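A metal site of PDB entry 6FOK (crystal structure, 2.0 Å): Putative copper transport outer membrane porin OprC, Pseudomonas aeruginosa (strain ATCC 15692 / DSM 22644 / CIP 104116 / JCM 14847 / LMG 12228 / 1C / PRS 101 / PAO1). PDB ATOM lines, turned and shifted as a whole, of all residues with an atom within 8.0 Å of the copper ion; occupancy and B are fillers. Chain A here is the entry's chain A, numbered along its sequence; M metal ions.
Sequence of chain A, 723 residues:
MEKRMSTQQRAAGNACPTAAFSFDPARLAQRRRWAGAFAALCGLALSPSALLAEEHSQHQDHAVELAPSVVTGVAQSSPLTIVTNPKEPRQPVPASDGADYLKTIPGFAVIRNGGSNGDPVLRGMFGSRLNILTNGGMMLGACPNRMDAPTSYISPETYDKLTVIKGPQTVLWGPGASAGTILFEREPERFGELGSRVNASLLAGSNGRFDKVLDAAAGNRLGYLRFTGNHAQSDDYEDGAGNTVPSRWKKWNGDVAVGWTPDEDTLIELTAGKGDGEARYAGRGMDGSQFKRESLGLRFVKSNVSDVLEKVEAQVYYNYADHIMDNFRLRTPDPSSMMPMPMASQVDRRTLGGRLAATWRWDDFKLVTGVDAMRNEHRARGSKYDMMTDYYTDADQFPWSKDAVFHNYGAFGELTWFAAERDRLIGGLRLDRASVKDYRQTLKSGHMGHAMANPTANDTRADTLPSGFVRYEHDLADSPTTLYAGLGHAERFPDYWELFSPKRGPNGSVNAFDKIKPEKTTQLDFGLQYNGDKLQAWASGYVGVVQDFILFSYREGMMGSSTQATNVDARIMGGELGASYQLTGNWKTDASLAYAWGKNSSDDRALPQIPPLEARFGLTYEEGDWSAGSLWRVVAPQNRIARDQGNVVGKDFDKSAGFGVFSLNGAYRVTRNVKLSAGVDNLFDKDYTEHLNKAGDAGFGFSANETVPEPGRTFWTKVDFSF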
ATOM      1  N   ALA A 142      24.405 -11.807  19.404  1.00  0.00           N
ATOM      2  CA  ALA A 142      23.816 -12.403  18.214  1.00  0.00           C
ATOM      3  C   ALA A 142      22.371 -12.857  18.389  1.00  0.00           C
ATOM      4  O   ALA A 142      21.680 -13.071  17.383  1.00  0.00           O
ATOM      5  CB  ALA A 142      24.661 -13.588  17.759  1.00  0.00           C
ATOM      6  N   CYS A 143      21.879 -13.026  19.624  1.00  0.00           N
ATOM      7  CA  CYS A 143      20.544 -13.626  19.784  1.00  0.00           C
ATOM      8  C   CYS A 143      19.474 -12.642  19.313  1.00  0.00           C
ATOM      9  O   CYS A 143      19.498 -11.470  19.722  1.00  0.00           O
ATOM     10  CB  CYS A 143      20.280 -14.031  21.232  1.00  0.00           C
ATOM     11  SG  CYS A 143      18.647 -14.786  21.480  1.00  0.00           S
ATOM     12  N   PRO A 144      18.526 -13.060  18.477  1.00  0.00           N
ATOM     13  CA  PRO A 144      17.465 -12.129  18.040  1.00  0.00           C
ATOM     14  C   PRO A 144      16.496 -11.732  19.146  1.00  0.00           C
ATOM     15  O   PRO A 144      15.763 -10.735  18.980  1.00  0.00           O
ATOM     16  CB  PRO A 144      16.741 -12.916  16.930  1.00  0.00           C
ATOM     17  CG  PRO A 144      17.012 -14.330  17.220  1.00  0.00           C
ATOM     18  CD  PRO A 144      18.429 -14.364  17.808  1.00  0.00           C
ATOM     19  N   ASN A 145      16.516 -12.438  20.286  1.00  0.00           N
ATOM     20  CA  ASN A 145      15.723 -12.084  21.456  1.00  0.00           C
ATOM     21  C   ASN A 145      16.605 -11.624  22.612  1.00  0.00           C
ATOM     22  O   ASN A 145      16.175 -11.664  23.774  1.00  0.00           O
ATOM     23  CB  ASN A 145      14.880 -13.280  21.877  1.00  0.00           C
ATOM     24  CG  ASN A 145      14.192 -13.953  20.690  1.00  0.00           C
ATOM     25  OD1 ASN A 145      13.297 -13.370  20.083  1.00  0.00           O
ATOM     26  ND2 ASN A 145      14.627 -15.174  20.364  1.00  0.00           N
ATOM     27  N   ARG A 146      17.844 -11.221  22.334  1.00  0.00           N
ATOM     28  CA  ARG A 146      18.742 -10.630  23.320  1.00  0.00           C
ATOM     29  C   ARG A 146      19.001 -11.539  24.518  1.00  0.00           C
ATOM     30  O   ARG A 146      19.091 -11.066  25.651  1.00  0.00           O
ATOM     31  CB  ARG A 146      18.225  -9.291  23.834  1.00  0.00           C
ATOM     32  CG  ARG A 146      17.705  -8.372  22.796  1.00  0.00           C
ATOM     33  CD  ARG A 146      18.540  -7.157  22.657  1.00  0.00           C
ATOM     34  NE  ARG A 146      19.092  -6.607  23.909  1.00  0.00           N
ATOM     35  CZ  ARG A 146      20.058  -5.679  23.893  1.00  0.00           C
ATOM     36  NH1 ARG A 146      20.516  -5.224  22.722  1.00  0.00           N
ATOM     37  NH2 ARG A 146      20.559  -5.185  25.018  1.00  0.00           N
ATOM     38  N   MET A 147      19.129 -12.851  24.281  1.00  0.00           N
ATOM     39  CA  MET A 147      19.648 -13.703  25.348  1.00  0.00           C
ATOM     40  C   MET A 147      21.063 -13.286  25.745  1.00  0.00           C
ATOM     41  O   MET A 147      21.459 -13.513  26.897  1.00  0.00           O
ATOM     42  CB  MET A 147      19.655 -15.165  24.929  1.00  0.00           C
ATOM     43  CG  MET A 147      18.289 -15.815  24.770  1.00  0.00           C
ATOM     44  SD  MET A 147      18.594 -17.523  24.277  1.00  0.00           S
ATOM     45  CE  MET A 147      16.929 -18.198  24.375  1.00  0.00           C
ATOM     46  N   ASP A 148      21.837 -12.713  24.821  1.00  0.00           N
ATOM     47  CA  ASP A 148      23.244 -12.353  25.086  1.00  0.00           C
ATOM     48  C   ASP A 148      23.454 -10.851  24.892  1.00  0.00           C
ATOM     49  O   ASP A 148      24.126 -10.435  23.936  1.00  0.00           O
ATOM     50  CB  ASP A 148      24.212 -13.169  24.190  1.00  0.00           C
ATOM     51  CG  ASP A 148      24.023 -12.907  22.688  1.00  0.00           C
ATOM     52  OD1 ASP A 148      22.913 -12.438  22.295  1.00  0.00           O
ATOM     53  OD2 ASP A 148      24.972 -13.168  21.913  1.00  0.00           O
ATOM     54  N   TYR A 281      16.795 -20.042  30.670  1.00  0.00           N
ATOM     55  CA  TYR A 281      16.021 -18.821  30.616  1.00  0.00           C
ATOM     56  C   TYR A 281      14.619 -19.117  31.122  1.00  0.00           C
ATOM     57  O   TYR A 281      13.902 -19.943  30.543  1.00  0.00           O
ATOM     58  CB  TYR A 281      16.000 -18.242  29.194  1.00  0.00           C
ATOM     59  CG  TYR A 281      17.323 -17.562  28.871  1.00  0.00           C
ATOM     60  CD1 TYR A 281      18.428 -18.301  28.504  1.00  0.00           C
ATOM     61  CD2 TYR A 281      17.469 -16.200  29.026  1.00  0.00           C
ATOM     62  CE1 TYR A 281      19.669 -17.669  28.257  1.00  0.00           C
ATOM     63  CE2 TYR A 281      18.695 -15.577  28.792  1.00  0.00           C
ATOM     64  CZ  TYR A 281      19.779 -16.315  28.416  1.00  0.00           C
ATOM     65  OH  TYR A 281      20.976 -15.687  28.205  1.00  0.00           O
ATOM     66  N   ARG A 284      11.017 -18.511  28.808  1.00  0.00           N
ATOM     67  CA  ARG A 284      11.274 -18.589  27.371  1.00  0.00           C
ATOM     68  C   ARG A 284      11.124 -20.033  26.900  1.00  0.00           C
ATOM     69  O   ARG A 284      11.280 -20.981  27.673  1.00  0.00           O
ATOM     70  CB  ARG A 284      12.674 -18.095  26.996  1.00  0.00           C
ATOM     71  CG  ARG A 284      12.857 -16.586  27.151  1.00  0.00           C
ATOM     72  CD  ARG A 284      14.284 -16.135  26.833  1.00  0.00           C
ATOM     73  NE  ARG A 284      14.570 -14.752  27.256  1.00  0.00           N
ATOM     74  CZ  ARG A 284      14.966 -13.796  26.419  1.00  0.00           C
ATOM     75  NH1 ARG A 284      15.088 -14.067  25.129  1.00  0.00           N
ATOM     76  NH2 ARG A 284      15.244 -12.567  26.864  1.00  0.00           N
ATOM     77  N   MET A 286      13.200 -21.443  24.881  1.00  0.00           N
ATOM     78  CA  MET A 286      14.518 -22.025  24.660  1.00  0.00           C
ATOM     79  C   MET A 286      15.498 -21.518  25.713  1.00  0.00           C
ATOM     80  O   MET A 286      15.314 -20.444  26.287  1.00  0.00           O
ATOM     81  CB  MET A 286      15.060 -21.664  23.274  1.00  0.00           C
ATOM     82  CG  MET A 286      14.377 -22.403  22.116  1.00  0.00           C
ATOM     83  SD  MET A 286      15.191 -21.933  20.575  1.00  0.00           S
ATOM     84  CE  MET A 286      14.309 -20.417  20.218  1.00  0.00           C
ATOM     85  N   ASP A 287      16.552 -22.284  25.923  1.00  0.00           N
ATOM     86  CA  ASP A 287      17.682 -21.891  26.730  1.00  0.00           C
ATOM     87  C   ASP A 287      18.864 -21.609  25.823  1.00  0.00           C
ATOM     88  O   ASP A 287      18.860 -21.976  24.643  1.00  0.00           O
ATOM     89  CB  ASP A 287      18.045 -22.997  27.728  1.00  0.00           C
ATOM     90  CG  ASP A 287      16.822 -23.502  28.489  1.00  0.00           C
ATOM     91  OD1 ASP A 287      16.185 -22.692  29.212  1.00  0.00           O
ATOM     92  OD2 ASP A 287      16.491 -24.703  28.333  1.00  0.00           O
ATOM     93  N   GLY A 288      19.886 -20.958  26.383  1.00  0.00           N
ATOM     94  CA  GLY A 288      21.120 -20.744  25.648  1.00  0.00           C
ATOM     95  C   GLY A 288      22.122 -21.817  25.987  1.00  0.00           C
ATOM     96  O   GLY A 288      22.696 -21.819  27.086  1.00  0.00           O
ATOM     97  N   SER A 289      22.335 -22.772  25.077  1.00  0.00           N
ATOM     98  CA  SER A 289      23.325 -23.813  25.318  1.00  0.00           C
ATOM     99  C   SER A 289      24.731 -23.406  24.923  1.00  0.00           C
ATOM    100  O   SER A 289      25.683 -24.107  25.275  1.00  0.00           O
ATOM    101  CB  SER A 289      22.944 -25.100  24.578  1.00  0.00           C
ATOM    102  OG  SER A 289      22.808 -24.870  23.191  1.00  0.00           O
ATOM    103  N   GLN A 290      24.914 -22.276  24.233  1.00  0.00           N
ATOM    104  CA  GLN A 290      26.252 -21.838  23.885  1.00  0.00           C
ATOM    105  C   GLN A 290      26.257 -20.335  23.715  1.00  0.00           C
ATOM    106  O   GLN A 290      25.321 -19.752  23.135  1.00  0.00           O
ATOM    107  CB  GLN A 290      26.748 -22.532  22.595  1.00  0.00           C
ATOM    108  CG  GLN A 290      28.026 -21.972  22.040  1.00  0.00           C
ATOM    109  CD  GLN A 290      28.452 -22.670  20.764  1.00  0.00           C
ATOM    110  OE1 GLN A 290      28.845 -23.836  20.794  1.00  0.00           O
ATOM    111  NE2 GLN A 290      28.390 -21.953  19.643  1.00  0.00           N
ATOM    112  N   PHE A 291      27.313 -19.708  24.216  1.00  0.00           N
ATOM    113  CA  PHE A 291      27.545 -18.275  24.068  1.00  0.00           C
ATOM    114  C   PHE A 291      29.037 -18.064  23.791  1.00  0.00           C
ATOM    115  O   PHE A 291      29.764 -17.504  24.594  1.00  0.00           O
ATOM    116  CB  PHE A 291      27.167 -17.481  25.324  1.00  0.00           C
ATOM    117  CG  PHE A 291      25.690 -17.468  25.636  1.00  0.00           C
ATOM    118  CD1 PHE A 291      24.865 -16.539  25.030  1.00  0.00           C
ATOM    119  CD2 PHE A 291      25.154 -18.355  26.543  1.00  0.00           C
ATOM    120  CE1 PHE A 291      23.505 -16.507  25.319  1.00  0.00           C
ATOM    121  CE2 PHE A 291      23.791 -18.337  26.849  1.00  0.00           C
ATOM    122  CZ  PHE A 291      22.970 -17.405  26.235  1.00  0.00           C
ATOM    123  N   HIS A 323      26.260 -18.020  19.029  1.00  0.00           N
ATOM    124  CA  HIS A 323      25.270 -18.349  20.040  1.00  0.00           C
ATOM    125  C   HIS A 323      24.392 -19.495  19.551  1.00  0.00           C
ATOM    126  O   HIS A 323      23.987 -19.523  18.382  1.00  0.00           O
ATOM    127  CB  HIS A 323      24.439 -17.094  20.363  1.00  0.00           C
ATOM    128  CG  HIS A 323      23.163 -17.353  21.102  1.00  0.00           C
ATOM    129  ND1 HIS A 323      23.118 -17.950  22.345  1.00  0.00           N
ATOM    130  CD2 HIS A 323      21.868 -17.068  20.780  1.00  0.00           C
ATOM    131  CE1 HIS A 323      21.870 -18.021  22.754  1.00  0.00           C
ATOM    132  NE2 HIS A 323      21.091 -17.488  21.835  1.00  0.00           N
ATOM    133  N   ILE A 324      24.120 -20.465  20.426  1.00  0.00           N
ATOM    134  CA  ILE A 324      23.166 -21.523  20.142  1.00  0.00           C
ATOM    135  C   ILE A 324      22.097 -21.521  21.209  1.00  0.00           C
ATOM    136  O   ILE A 324      22.422 -21.515  22.405  1.00  0.00           O
ATOM    137  CB  ILE A 324      23.821 -22.906  20.045  1.00  0.00           C
ATOM    138  CG1 ILE A 324      24.813 -22.923  18.884  1.00  0.00           C
ATOM    139  CG2 ILE A 324      22.746 -23.977  19.851  1.00  0.00           C
ATOM    140  CD1 ILE A 324      25.600 -24.221  18.766  1.00  0.00           C
ATOM    141  N   MET A 325      20.836 -21.511  20.793  1.00  0.00           N
ATOM    142  CA  MET A 325      19.716 -21.759  21.692  1.00  0.00           C
ATOM    143  C   MET A 325      18.911 -22.956  21.209  1.00  0.00           C
ATOM    144  O   MET A 325      18.833 -23.226  20.002  1.00  0.00           O
ATOM    145  CB  MET A 325      18.813 -20.547  21.826  1.00  0.00           C
ATOM    146  CG  MET A 325      18.463 -19.879  20.523  1.00  0.00           C
ATOM    147  SD  MET A 325      17.580 -18.344  20.833  1.00  0.00           S
ATOM    148  CE  MET A 325      17.359 -17.795  19.126  1.00  0.00           C
ATOM    149  N   ASP A 326      18.305 -23.678  22.154  1.00  0.00           N
ATOM    150  CA  ASP A 326      17.539 -24.883  21.832  1.00  0.00           C
ATOM    151  C   ASP A 326      16.621 -25.214  23.007  1.00  0.00           C
ATOM    152  O   ASP A 326      16.699 -24.608  24.082  1.00  0.00           O
ATOM    153  CB  ASP A 326      18.466 -26.051  21.506  1.00  0.00           C
ATOM    154  CG  ASP A 326      19.306 -26.458  22.688  1.00  0.00           C
ATOM    155  OD1 ASP A 326      18.745 -26.918  23.712  1.00  0.00           O
ATOM    156  OD2 ASP A 326      20.561 -26.327  22.589  1.00  0.00           O
ATOM    157  N   SER A 345      18.288 -23.029  17.217  1.00  0.00           N
ATOM    158  CA  SER A 345      18.706 -21.946  16.336  1.00  0.00           C
ATOM    159  C   SER A 345      20.123 -21.560  16.691  1.00  0.00           C
ATOM    160  O   SER A 345      20.471 -21.438  17.873  1.00  0.00           O
ATOM    161  CB  SER A 345      17.806 -20.721  16.475  1.00  0.00           C
ATOM    162  OG  SER A 345      16.449 -21.121  16.467  1.00  0.00           O
ATOM    163  N   GLN A 346      20.959 -21.360  15.669  1.00  0.00           N
ATOM    164  CA  GLN A 346      22.313 -20.855  15.850  1.00  0.00           C
ATOM    165  C   GLN A 346      22.433 -19.518  15.123  1.00  0.00           C
ATOM    166  O   GLN A 346      21.887 -19.352  14.024  1.00  0.00           O
ATOM    167  CB  GLN A 346      23.336 -21.861  15.341  1.00  0.00           C
ATOM    168  CG  GLN A 346      24.799 -21.398  15.502  1.00  0.00           C
ATOM    169  CD  GLN A 346      25.769 -22.497  15.191  1.00  0.00           C
ATOM    170  OE1 GLN A 346      25.424 -23.469  14.497  1.00  0.00           O
ATOM    171  NE2 GLN A 346      26.996 -22.370  15.697  1.00  0.00           N
ATOM    172  N   VAL A 347      23.108 -18.569  15.751  1.00  0.00           N
ATOM    173  CA  VAL A 347      23.211 -17.204  15.249  1.00  0.00           C
ATOM    174  C   VAL A 347      24.604 -16.717  15.577  1.00  0.00           C
ATOM    175  O   VAL A 347      25.195 -17.094  16.592  1.00  0.00           O
ATOM    176  CB  VAL A 347      22.152 -16.244  15.842  1.00  0.00           C
ATOM    177  CG1 VAL A 347      20.758 -16.540  15.296  1.00  0.00           C
ATOM    178  CG2 VAL A 347      22.146 -16.319  17.401  1.00  0.00           C
HETATM  179 CU    CU M   1      19.052 -16.930  21.920  1.00  0.00          CU
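N of His 323 is in hydrogen-bond range of O of Val 347, at 2.8 Å.
A ring nitrogen (ND1) of His 323 sits at hydrogen-bond distance from the backbone carbonyl oxygen of Gln 290.
The side-chain sulfur (SG) of Cys 143 sits close to the backbone NH (N) of Asn 145, 3.4 Å away.
OD1 of Asp 148 is in hydrogen-bond range of N of Cys 143.
The side-chain sulfur (SG) of Cys 143 sits close to the backbone NH (N) of Arg 146 (3.8 Å).
The backbone NH (N) of Ser 345 lies within hydrogen-bond range of the backbone carbonyl oxygen (O) of Met 325, 2.8 Å away.
The side-chain hydroxyl (OH) of Tyr 281 sits at hydrogen-bond distance from the backbone carbonyl oxygen (O) of Met 147 (2.6 Å).
Four residues have an atom within 4 Å of the copper ion: Cys 143, Met 147, His 323 and Met 325.
The copper ion is bound by NE2 of His 323 (2.1 Å), SG of Cys 143 (2.2 Å), SD of Met 325 (2.3 Å) and SD of Met 147 (2.5 Å).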
